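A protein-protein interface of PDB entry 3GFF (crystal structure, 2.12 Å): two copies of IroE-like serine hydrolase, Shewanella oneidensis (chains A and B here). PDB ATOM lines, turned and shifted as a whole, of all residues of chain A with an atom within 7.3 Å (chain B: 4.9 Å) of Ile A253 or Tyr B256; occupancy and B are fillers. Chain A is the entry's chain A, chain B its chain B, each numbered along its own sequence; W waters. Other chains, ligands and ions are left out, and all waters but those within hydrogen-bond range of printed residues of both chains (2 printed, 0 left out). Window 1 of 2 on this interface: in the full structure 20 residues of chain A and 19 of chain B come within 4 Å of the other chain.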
ATOM      1  N   HIS A  57      16.823  -3.825  -6.224  1.00  0.00           N
ATOM      2  CA  HIS A  57      15.803  -4.888  -6.240  1.00  0.00           C
ATOM      3  C   HIS A  57      15.019  -4.892  -7.536  1.00  0.00           C
ATOM      4  O   HIS A  57      14.598  -5.956  -7.981  1.00  0.00           O
ATOM      5  CB  HIS A  57      14.840  -4.849  -5.020  1.00  0.00           C
ATOM      6  CG  HIS A  57      13.797  -3.770  -5.084  1.00  0.00           C
ATOM      7  ND1 HIS A  57      12.503  -4.000  -5.510  1.00  0.00           N
ATOM      8  CD2 HIS A  57      13.849  -2.462  -4.744  1.00  0.00           C
ATOM      9  CE1 HIS A  57      11.816  -2.870  -5.469  1.00  0.00           C
ATOM     10  NE2 HIS A  57      12.608  -1.922  -5.004  1.00  0.00           N
ATOM     11  N   LEU A  61      15.090  -7.982 -10.337  1.00  0.00           N
ATOM     12  CA  LEU A  61      13.826  -8.573 -10.730  1.00  0.00           C
ATOM     13  C   LEU A  61      13.739  -8.525 -12.263  1.00  0.00           C
ATOM     14  O   LEU A  61      13.506  -9.540 -12.912  1.00  0.00           O
ATOM     15  CB  LEU A  61      12.662  -7.861 -10.028  1.00  0.00           C
ATOM     16  CG  LEU A  61      11.257  -8.223 -10.510  1.00  0.00           C
ATOM     17  CD1 LEU A  61      11.045  -9.755 -10.329  1.00  0.00           C
ATOM     18  CD2 LEU A  61      10.171  -7.360  -9.835  1.00  0.00           C
ATOM     19  N   LEU A 168       3.653   3.593  -9.359  1.00  0.00           N
ATOM     20  CA  LEU A 168       3.555   2.687  -8.211  1.00  0.00           C
ATOM     21  C   LEU A 168       3.263   3.453  -6.903  1.00  0.00           C
ATOM     22  O   LEU A 168       4.126   4.072  -6.298  1.00  0.00           O
ATOM     23  CB  LEU A 168       4.837   1.849  -8.107  1.00  0.00           C
ATOM     24  CG  LEU A 168       5.305   1.185  -9.433  1.00  0.00           C
ATOM     25  CD1 LEU A 168       6.656   0.410  -9.285  1.00  0.00           C
ATOM     26  CD2 LEU A 168       4.177   0.319 -10.002  1.00  0.00           C
ATOM     27  N   PHE A 198       0.129   1.999 -16.140  1.00  0.00           N
ATOM     28  CA  PHE A 198      -0.198   0.946 -15.164  1.00  0.00           C
ATOM     29  C   PHE A 198      -0.110   1.605 -13.822  1.00  0.00           C
ATOM     30  O   PHE A 198       0.892   2.278 -13.527  1.00  0.00           O
ATOM     31  CB  PHE A 198       0.785  -0.235 -15.241  1.00  0.00           C
ATOM     32  CG  PHE A 198       0.652  -1.229 -14.095  1.00  0.00           C
ATOM     33  CD1 PHE A 198      -0.253  -2.274 -14.163  1.00  0.00           C
ATOM     34  CD2 PHE A 198       1.461  -1.115 -12.973  1.00  0.00           C
ATOM     35  CE1 PHE A 198      -0.377  -3.188 -13.133  1.00  0.00           C
ATOM     36  CE2 PHE A 198       1.356  -2.017 -11.943  1.00  0.00           C
ATOM     37  CZ  PHE A 198       0.420  -3.059 -12.018  1.00  0.00           C
ATOM     38  N   ALA A 200      -0.184   0.830  -9.648  1.00  0.00           N
ATOM     39  CA  ALA A 200      -0.187  -0.127  -8.531  1.00  0.00           C
ATOM     40  C   ALA A 200      -0.765   0.700  -7.406  1.00  0.00           C
ATOM     41  O   ALA A 200      -0.379   1.865  -7.250  1.00  0.00           O
ATOM     42  CB  ALA A 200       1.239  -0.614  -8.153  1.00  0.00           C
ATOM     43  N   LYS A 240      -4.003  -2.227 -10.405  1.00  0.00           N
ATOM     44  CA  LYS A 240      -4.153  -3.363  -9.512  1.00  0.00           C
ATOM     45  C   LYS A 240      -4.021  -2.861  -8.088  1.00  0.00           C
ATOM     46  O   LYS A 240      -3.107  -2.122  -7.775  1.00  0.00           O
ATOM     47  CB  LYS A 240      -3.166  -4.501  -9.802  1.00  0.00           C
ATOM     48  CG  LYS A 240      -3.338  -5.691  -8.818  1.00  0.00           C
ATOM     49  CD  LYS A 240      -2.461  -6.920  -9.093  1.00  0.00           C
ATOM     50  CE  LYS A 240      -3.191  -8.046  -9.837  1.00  0.00           C
ATOM     51  NZ  LYS A 240      -2.271  -9.206  -9.996  1.00  0.00           N
ATOM     52  N   TYR A 242      -3.531  -3.747  -4.095  1.00  0.00           N
ATOM     53  CA  TYR A 242      -2.823  -4.714  -3.255  1.00  0.00           C
ATOM     54  C   TYR A 242      -3.160  -4.495  -1.770  1.00  0.00           C
ATOM     55  O   TYR A 242      -2.460  -3.749  -1.066  1.00  0.00           O
ATOM     56  CB  TYR A 242      -1.310  -4.546  -3.461  1.00  0.00           C
ATOM     57  CG  TYR A 242      -0.813  -4.783  -4.886  1.00  0.00           C
ATOM     58  CD1 TYR A 242      -0.733  -3.746  -5.803  1.00  0.00           C
ATOM     59  CD2 TYR A 242      -0.375  -6.047  -5.285  1.00  0.00           C
ATOM     60  CE1 TYR A 242      -0.263  -3.969  -7.093  1.00  0.00           C
ATOM     61  CE2 TYR A 242       0.085  -6.282  -6.539  1.00  0.00           C
ATOM     62  CZ  TYR A 242       0.163  -5.232  -7.441  1.00  0.00           C
ATOM     63  OH  TYR A 242       0.604  -5.500  -8.708  1.00  0.00           O
ATOM     64  N   GLU A 244      -2.628  -6.267   0.779  1.00  0.00           N
ATOM     65  CA  GLU A 244      -1.613  -6.774   1.706  1.00  0.00           C
ATOM     66  C   GLU A 244      -0.282  -6.115   1.486  1.00  0.00           C
ATOM     67  O   GLU A 244       0.722  -6.638   1.878  1.00  0.00           O
ATOM     68  CB  GLU A 244      -1.493  -8.292   1.590  1.00  0.00           C
ATOM     69  CG  GLU A 244      -2.839  -9.040   1.669  1.00  0.00           C
ATOM     70  CD  GLU A 244      -3.628  -8.733   2.928  1.00  0.00           C
ATOM     71  OE1 GLU A 244      -2.996  -8.513   3.985  1.00  0.00           O
ATOM     72  OE2 GLU A 244      -4.893  -8.718   2.871  1.00  0.00           O
ATOM     73  N   GLU A 245      -0.262  -4.974   0.809  1.00  0.00           N
ATOM     74  CA  GLU A 245       0.961  -4.244   0.627  1.00  0.00           C
ATOM     75  C   GLU A 245       0.875  -2.844   1.247  1.00  0.00           C
ATOM     76  O   GLU A 245      -0.229  -2.268   1.468  1.00  0.00           O
ATOM     77  CB  GLU A 245       1.317  -4.119  -0.871  1.00  0.00           C
ATOM     78  CG  GLU A 245       1.545  -5.471  -1.624  1.00  0.00           C
ATOM     79  CD  GLU A 245       2.789  -6.216  -1.204  1.00  0.00           C
ATOM     80  OE1 GLU A 245       3.790  -5.598  -0.779  1.00  0.00           O
ATOM     81  OE2 GLU A 245       2.775  -7.447  -1.320  1.00  0.00           O
ATOM     82  N   SER A 249       6.386  -1.194   0.406  1.00  0.00           N
ATOM     83  CA  SER A 249       6.554  -2.588  -0.132  1.00  0.00           C
ATOM     84  C   SER A 249       5.969  -2.842  -1.530  1.00  0.00           C
ATOM     85  O   SER A 249       6.306  -3.835  -2.174  1.00  0.00           O
ATOM     86  CB  SER A 249       5.951  -3.643   0.798  1.00  0.00           C
ATOM     87  OG  SER A 249       4.545  -3.780   0.606  1.00  0.00           O
ATOM     88  N   VAL A 250       5.080  -1.983  -1.990  1.00  0.00           N
ATOM     89  CA  VAL A 250       4.425  -2.253  -3.263  1.00  0.00           C
ATOM     90  C   VAL A 250       5.307  -1.943  -4.481  1.00  0.00           C
ATOM     91  O   VAL A 250       4.965  -2.347  -5.590  1.00  0.00           O
ATOM     92  CB  VAL A 250       3.054  -1.540  -3.383  1.00  0.00           C
ATOM     93  CG1 VAL A 250       3.251  -0.060  -3.823  1.00  0.00           C
ATOM     94  CG2 VAL A 250       2.148  -2.300  -4.372  1.00  0.00           C
ATOM     95  N   SER A 251       6.452  -1.276  -4.277  1.00  0.00           N
ATOM     96  CA  SER A 251       7.351  -0.940  -5.383  1.00  0.00           C
ATOM     97  C   SER A 251       7.756  -2.185  -6.134  1.00  0.00           C
ATOM     98  O   SER A 251       7.738  -2.218  -7.387  1.00  0.00           O
ATOM     99  CB  SER A 251       8.599  -0.146  -4.902  1.00  0.00           C
ATOM    100  OG  SER A 251       9.427  -0.894  -4.003  1.00  0.00           O
ATOM    101  N   HIS A 252       8.050  -3.236  -5.378  1.00  0.00           N
ATOM    102  CA  HIS A 252       8.523  -4.490  -5.968  1.00  0.00           C
ATOM    103  C   HIS A 252       7.467  -5.294  -6.753  1.00  0.00           C
ATOM    104  O   HIS A 252       7.687  -5.572  -7.952  1.00  0.00           O
ATOM    105  CB  HIS A 252       9.136  -5.361  -4.900  1.00  0.00           C
ATOM    106  CG  HIS A 252       9.944  -6.505  -5.439  1.00  0.00           C
ATOM    107  ND1 HIS A 252      11.266  -6.368  -5.805  1.00  0.00           N
ATOM    108  CD2 HIS A 252       9.633  -7.807  -5.624  1.00  0.00           C
ATOM    109  CE1 HIS A 252      11.732  -7.539  -6.205  1.00  0.00           C
ATOM    110  NE2 HIS A 252      10.763  -8.433  -6.095  1.00  0.00           N
ATOM    111  N   ILE A 253       6.383  -5.707  -6.075  1.00  0.00           N
ATOM    112  CA  ILE A 253       5.298  -6.496  -6.693  1.00  0.00           C
ATOM    113  C   ILE A 253       4.569  -5.661  -7.739  1.00  0.00           C
ATOM    114  O   ILE A 253       3.980  -6.213  -8.680  1.00  0.00           O
ATOM    115  CB  ILE A 253       4.277  -7.129  -5.617  1.00  0.00           C
ATOM    116  CG1 ILE A 253       3.516  -8.332  -6.200  1.00  0.00           C
ATOM    117  CG2 ILE A 253       3.297  -6.095  -5.051  1.00  0.00           C
ATOM    118  CD1 ILE A 253       4.426  -9.526  -6.731  1.00  0.00           C
ATOM    119  N   GLY A 254       4.582  -4.333  -7.550  1.00  0.00           N
ATOM    120  CA  GLY A 254       3.972  -3.380  -8.492  1.00  0.00           C
ATOM    121  C   GLY A 254       4.702  -3.393  -9.832  1.00  0.00           C
ATOM    122  O   GLY A 254       4.071  -3.404 -10.886  1.00  0.00           O
ATOM    123  N   LEU A 255       6.035  -3.392  -9.791  1.00  0.00           N
ATOM    124  CA  LEU A 255       6.854  -3.524 -11.002  1.00  0.00           C
ATOM    125  C   LEU A 255       6.696  -4.960 -11.542  1.00  0.00           C
ATOM    126  O   LEU A 255       6.530  -5.182 -12.726  1.00  0.00           O
ATOM    127  CB  LEU A 255       8.332  -3.249 -10.691  1.00  0.00           C
ATOM    128  CG  LEU A 255       9.374  -3.420 -11.831  1.00  0.00           C
ATOM    129  CD1 LEU A 255       9.234  -2.354 -12.952  1.00  0.00           C
ATOM    130  CD2 LEU A 255      10.840  -3.408 -11.260  1.00  0.00           C
ATOM    131  N   TYR A 256       6.736  -5.947 -10.657  1.00  0.00           N
ATOM    132  CA  TYR A 256       6.565  -7.314 -11.083  1.00  0.00           C
ATOM    133  C   TYR A 256       5.328  -7.449 -11.986  1.00  0.00           C
ATOM    134  O   TYR A 256       5.410  -7.904 -13.132  1.00  0.00           O
ATOM    135  CB  TYR A 256       6.475  -8.233  -9.883  1.00  0.00           C
ATOM    136  CG  TYR A 256       6.472  -9.704 -10.245  1.00  0.00           C
ATOM    137  CD1 TYR A 256       5.289 -10.367 -10.590  1.00  0.00           C
ATOM    138  CD2 TYR A 256       7.653 -10.443 -10.235  1.00  0.00           C
ATOM    139  CE1 TYR A 256       5.296 -11.742 -10.927  1.00  0.00           C
ATOM    140  CE2 TYR A 256       7.673 -11.774 -10.585  1.00  0.00           C
ATOM    141  CZ  TYR A 256       6.499 -12.433 -10.938  1.00  0.00           C
ATOM    142  OH  TYR A 256       6.547 -13.791 -11.255  1.00  0.00           O
ATOM    143  N   ASP A 257       4.184  -6.986 -11.505  1.00  0.00           N
ATOM    144  CA  ASP A 257       2.951  -7.172 -12.250  1.00  0.00           C
ATOM    145  C   ASP A 257       2.810  -6.187 -13.369  1.00  0.00           C
ATOM    146  O   ASP A 257       2.175  -6.504 -14.410  1.00  0.00           O
ATOM    147  CB  ASP A 257       1.763  -7.035 -11.341  1.00  0.00           C
ATOM    148  CG  ASP A 257       1.637  -8.155 -10.388  1.00  0.00           C
ATOM    149  OD1 ASP A 257       2.025  -9.319 -10.734  1.00  0.00           O
ATOM    150  OD2 ASP A 257       1.070  -7.860  -9.301  1.00  0.00           O
ATOM    151  N   GLY A 258       3.358  -4.991 -13.155  1.00  0.00           N
ATOM    152  CA  GLY A 258       3.280  -3.933 -14.148  1.00  0.00           C
ATOM    153  C   GLY A 258       4.053  -4.255 -15.405  1.00  0.00           C
ATOM    154  O   GLY A 258       3.536  -4.109 -16.491  1.00  0.00           O
ATOM    155  N   ILE A 259       5.284  -4.722 -15.241  1.00  0.00           N
ATOM    156  CA  ILE A 259       6.193  -5.003 -16.366  1.00  0.00           C
ATOM    157  C   ILE A 259       5.800  -6.267 -17.103  1.00  0.00           C
ATOM    158  O   ILE A 259       6.040  -6.361 -18.305  1.00  0.00           O
ATOM    159  CB  ILE A 259       7.699  -5.075 -15.901  1.00  0.00           C
ATOM    160  CG1 ILE A 259       8.630  -4.633 -17.037  1.00  0.00           C
ATOM    161  CG2 ILE A 259       8.040  -6.432 -15.319  1.00  0.00           C
ATOM    162  CD1 ILE A 259       8.395  -3.130 -17.456  1.00  0.00           C
ATOM    163  N   LEU B  61      15.427  -9.667  -2.615  1.00  0.00           N
ATOM    164  CA  LEU B  61      14.018  -9.630  -2.265  1.00  0.00           C
ATOM    165  C   LEU B  61      13.838  -9.752  -0.758  1.00  0.00           C
ATOM    166  O   LEU B  61      13.090  -8.982  -0.135  1.00  0.00           O
ATOM    167  CB  LEU B  61      13.287 -10.787  -2.960  1.00  0.00           C
ATOM    168  CG  LEU B  61      11.833 -10.998  -2.564  1.00  0.00           C
ATOM    169  CD1 LEU B  61      11.025  -9.712  -2.885  1.00  0.00           C
ATOM    170  CD2 LEU B  61      11.279 -12.286  -3.240  1.00  0.00           C
ATOM    171  N   LEU B  65      11.994  -6.941   1.583  1.00  0.00           N
ATOM    172  CA  LEU B  65      10.794  -7.272   2.347  1.00  0.00           C
ATOM    173  C   LEU B  65      10.981  -6.968   3.836  1.00  0.00           C
ATOM    174  O   LEU B  65      10.017  -6.737   4.515  1.00  0.00           O
ATOM    175  CB  LEU B  65      10.417  -8.752   2.190  1.00  0.00           C
ATOM    176  CG  LEU B  65       9.837  -9.276   0.862  1.00  0.00           C
ATOM    177  CD1 LEU B  65       9.812 -10.758   0.776  1.00  0.00           C
ATOM    178  CD2 LEU B  65       8.458  -8.705   0.636  1.00  0.00           C
ATOM    179  N   HIS B 252      11.293 -16.819  -7.904  1.00  0.00           N
ATOM    180  CA  HIS B 252      11.137 -15.482  -7.335  1.00  0.00           C
ATOM    181  C   HIS B 252       9.734 -15.284  -6.695  1.00  0.00           C
ATOM    182  O   HIS B 252       9.639 -15.067  -5.522  1.00  0.00           O
ATOM    183  CB  HIS B 252      11.393 -14.392  -8.386  1.00  0.00           C
ATOM    184  CG  HIS B 252      11.586 -13.026  -7.793  1.00  0.00           C
ATOM    185  ND1 HIS B 252      12.813 -12.576  -7.359  1.00  0.00           N
ATOM    186  CD2 HIS B 252      10.705 -12.032  -7.516  1.00  0.00           C
ATOM    187  CE1 HIS B 252      12.688 -11.352  -6.876  1.00  0.00           C
ATOM    188  NE2 HIS B 252      11.421 -11.004  -6.950  1.00  0.00           N
ATOM    189  N   ILE B 253       8.654 -15.384  -7.477  1.00  0.00           N
ATOM    190  CA  ILE B 253       7.328 -15.205  -6.905  1.00  0.00           C
ATOM    191  C   ILE B 253       7.036 -16.281  -5.859  1.00  0.00           C
ATOM    192  O   ILE B 253       6.349 -15.990  -4.885  1.00  0.00           O
ATOM    193  CB  ILE B 253       6.236 -15.121  -7.992  1.00  0.00           C
ATOM    194  CG1 ILE B 253       4.947 -14.482  -7.448  1.00  0.00           C
ATOM    195  CG2 ILE B 253       5.995 -16.496  -8.653  1.00  0.00           C
ATOM    196  CD1 ILE B 253       4.997 -12.928  -7.208  1.00  0.00           C
ATOM    197  N   GLY B 254       7.519 -17.517  -6.056  1.00  0.00           N
ATOM    198  CA  GLY B 254       7.302 -18.595  -5.078  1.00  0.00           C
ATOM    199  C   GLY B 254       7.918 -18.248  -3.723  1.00  0.00           C
ATOM    200  O   GLY B 254       7.322 -18.452  -2.637  1.00  0.00           O
ATOM    201  N   LEU B 255       9.138 -17.726  -3.767  1.00  0.00           N
ATOM    202  CA  LEU B 255       9.777 -17.280  -2.539  1.00  0.00           C
ATOM    203  C   LEU B 255       8.965 -16.113  -1.953  1.00  0.00           C
ATOM    204  O   LEU B 255       8.713 -16.074  -0.745  1.00  0.00           O
ATOM    205  CB  LEU B 255      11.240 -16.870  -2.794  1.00  0.00           C
ATOM    206  CG  LEU B 255      11.966 -16.210  -1.606  1.00  0.00           C
ATOM    207  CD1 LEU B 255      12.013 -17.126  -0.417  1.00  0.00           C
ATOM    208  CD2 LEU B 255      13.384 -15.708  -2.018  1.00  0.00           C
ATOM    209  N   TYR B 256       8.531 -15.196  -2.810  1.00  0.00           N
ATOM    210  CA  TYR B 256       7.780 -13.997  -2.352  1.00  0.00           C
ATOM    211  C   TYR B 256       6.607 -14.350  -1.449  1.00  0.00           C
ATOM    212  O   TYR B 256       6.520 -13.907  -0.292  1.00  0.00           O
ATOM    213  CB  TYR B 256       7.288 -13.172  -3.555  1.00  0.00           C
ATOM    214  CG  TYR B 256       6.635 -11.822  -3.219  1.00  0.00           C
ATOM    215  CD1 TYR B 256       5.255 -11.703  -3.011  1.00  0.00           C
ATOM    216  CD2 TYR B 256       7.392 -10.650  -3.191  1.00  0.00           C
ATOM    217  CE1 TYR B 256       4.665 -10.461  -2.711  1.00  0.00           C
ATOM    218  CE2 TYR B 256       6.813  -9.419  -2.893  1.00  0.00           C
ATOM    219  CZ  TYR B 256       5.453  -9.331  -2.650  1.00  0.00           C
ATOM    220  OH  TYR B 256       4.908  -8.095  -2.367  1.00  0.00           O
ATOM    221  N   ASP B 257       5.729 -15.159  -2.017  1.00  0.00           N
ATOM    222  CA  ASP B 257       4.527 -15.605  -1.382  1.00  0.00           C
ATOM    223  C   ASP B 257       4.794 -16.572  -0.223  1.00  0.00           C
ATOM    224  O   ASP B 257       4.087 -16.534   0.775  1.00  0.00           O
ATOM    225  CB  ASP B 257       3.634 -16.283  -2.420  1.00  0.00           C
ATOM    226  CG  ASP B 257       3.034 -15.315  -3.415  1.00  0.00           C
ATOM    227  OD1 ASP B 257       2.718 -14.186  -3.049  1.00  0.00           O
ATOM    228  OD2 ASP B 257       2.801 -15.722  -4.574  1.00  0.00           O
ATOM    229  N   GLY B 258       5.763 -17.464  -0.375  1.00  0.00           N
ATOM    230  CA  GLY B 258       6.090 -18.431   0.669  1.00  0.00           C
ATOM    231  C   GLY B 258       6.671 -17.788   1.916  1.00  0.00           C
ATOM    232  O   GLY B 258       6.351 -18.197   3.028  1.00  0.00           O
ATOM    233  N   ILE B 259       7.552 -16.798   1.746  1.00  0.00           N
ATOM    234  CA  ILE B 259       8.209 -16.184   2.874  1.00  0.00           C
ATOM    235  C   ILE B 259       7.263 -15.203   3.551  1.00  0.00           C
ATOM    236  O   ILE B 259       7.243 -15.086   4.772  1.00  0.00           O
ATOM    237  CB  ILE B 259       9.551 -15.552   2.479  1.00  0.00           C
ATOM    238  CG1 ILE B 259      10.493 -15.573   3.676  1.00  0.00           C
ATOM    239  CG2 ILE B 259       9.381 -14.165   1.737  1.00  0.00           C
ATOM    240  CD1 ILE B 259      10.948 -17.004   4.056  1.00  0.00           C
ATOM    241  N   ARG B 260       6.439 -14.519   2.761  1.00  0.00           N
ATOM    242  CA  ARG B 260       5.434 -13.622   3.325  1.00  0.00           C
ATOM    243  C   ARG B 260       4.380 -14.428   4.132  1.00  0.00           C
ATOM    244  O   ARG B 260       3.954 -14.013   5.212  1.00  0.00           O
ATOM    245  CB  ARG B 260       4.831 -12.743   2.231  1.00  0.00           C
ATOM    246  CG  ARG B 260       5.730 -11.588   1.822  1.00  0.00           C
ATOM    247  CD  ARG B 260       5.238 -10.873   0.595  1.00  0.00           C
ATOM    248  NE  ARG B 260       3.812 -10.611   0.675  1.00  0.00           N
ATOM    249  CZ  ARG B 260       3.240  -9.536   1.226  1.00  0.00           C
ATOM    250  NH1 ARG B 260       3.959  -8.552   1.756  1.00  0.00           N
ATOM    251  NH2 ARG B 260       1.919  -9.464   1.255  1.00  0.00           N
HETATM  252  O   HOH W   1       8.668 -14.971 -10.256  1.00  0.00           O
HETATM  253  O   HOH W   2       6.357  -6.291  -3.223  1.00  0.00           O
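Water W2 lies within hydrogen-bond range of OH of Tyr B256, O of Ser A249 and N of Ile A253. Water W1 lies within hydrogen-bond range of the side-chain hydroxyl of Tyr A256 (2.6 Å) and the backbone NH of Ile B253 (2.8 Å).
Printed residues of chain B within 4 Å of Glu A244: Arg B260. Printed residues of chain B within 4 Å of His A252: Leu B61 (3.5 Å) and His B252 (2.8 Å). Ile A253 touches just these residues of chain B: Ile B253 (3.5 Å) and Tyr B256 (3.4 Å). Of the printed residues of chain A, His B252 touches Leu A61 and His A252. Of the printed residues of chain A, Ile B253 touches Ile A253 (3.5 Å) and Tyr A256 (3.5 Å). Of chain A, only Glu A245 and Ile A253 come within 4 Å of Tyr B256. The nearest printed residue of chain B that does not touch Ile A253 is Asp B257 (6.2 Å).
Leu A61 touches His B252, and with the chains exchanged His A252 touches Leu B61. His A252 touches its own counterpart, His B252. Ile A253 touches its own counterpart, Ile B253. Ile A253 touches Tyr B256, and with the chains exchanged Tyr A256 touches Ile B253. Positions printed for both chains: 61, 252, 253, 254, 255, 256, 257, 258 and 259.
The guanidinium group (NH2) of Arg B260 sits at hydrogen-bond distance from the backbone carbonyl oxygen (O) of Glu A244 (3.1 Å). The side-chain carboxylate (OE2) of Glu A245 lies within hydrogen-bond range of the side-chain hydroxyl (OH) of Tyr B256. The guanidinium group (NH2) of Arg B260 is in salt-bridge range of the side-chain carboxylate (OE2) of Glu A245 (3.4 Å). A ring nitrogen (NE2) of His A252 lies within hydrogen-bond range of a ring nitrogen (NE2) of His B252 (2.8 Å).
ND1 of His A252 lies within hydrogen-bond range of ND1 of His A57 (2.7 Å). The side-chain hydroxyl of Tyr A242 lies within hydrogen-bond range of the backbone carbonyl oxygen of Ile A253 (3.5 Å). The side-chain carboxylate (OE1) of Glu A245 lies within hydrogen-bond range of the side-chain hydroxyl (OG) of Ser A249, at 2.4 Å.
Leu A61 touches His B252. His A252 touches Leu B61 (NE2 to CD1, 3.5 Å). Ile A253 touches Ile B253 (CD1 to CD1, 3.5 Å). Ile A253 touches Tyr B256 (CB to OH, 3.4 Å). CB of Ile B253 touches OH of Tyr A256, at 3.5 Å.
Printed residues of chain B that touch a printed residue of chain A: Leu B61, His B252, Ile B253, Tyr B256 and Arg B260. Hydrophobic or aromatic side chains of chain B within 4 Å of the printed part of chain A: Leu B61, His B252, Ile B253 and Tyr B256. Of the 20 printed residues of chain A, 6 touch a printed residue of chain B. Printed residues of chain A that touch a printed residue of chain B: Leu A61, Glu A244, Glu A245, His A252, Ile A253 and Tyr A256. Hydrophobic or aromatic side chains of chain A within 4 Å of the printed part of chain B: Leu A61, His A252, Ile A253 and Tyr A256. Along chain A the printed residues that touch a printed residue of chain B span positions 61 to 256. Among the printed residues, Asp or Glu carboxylates within 4 Å of a Lys or Arg side-chain nitrogen of the other chain: Glu A245 with Arg B260 (3.4 Å).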
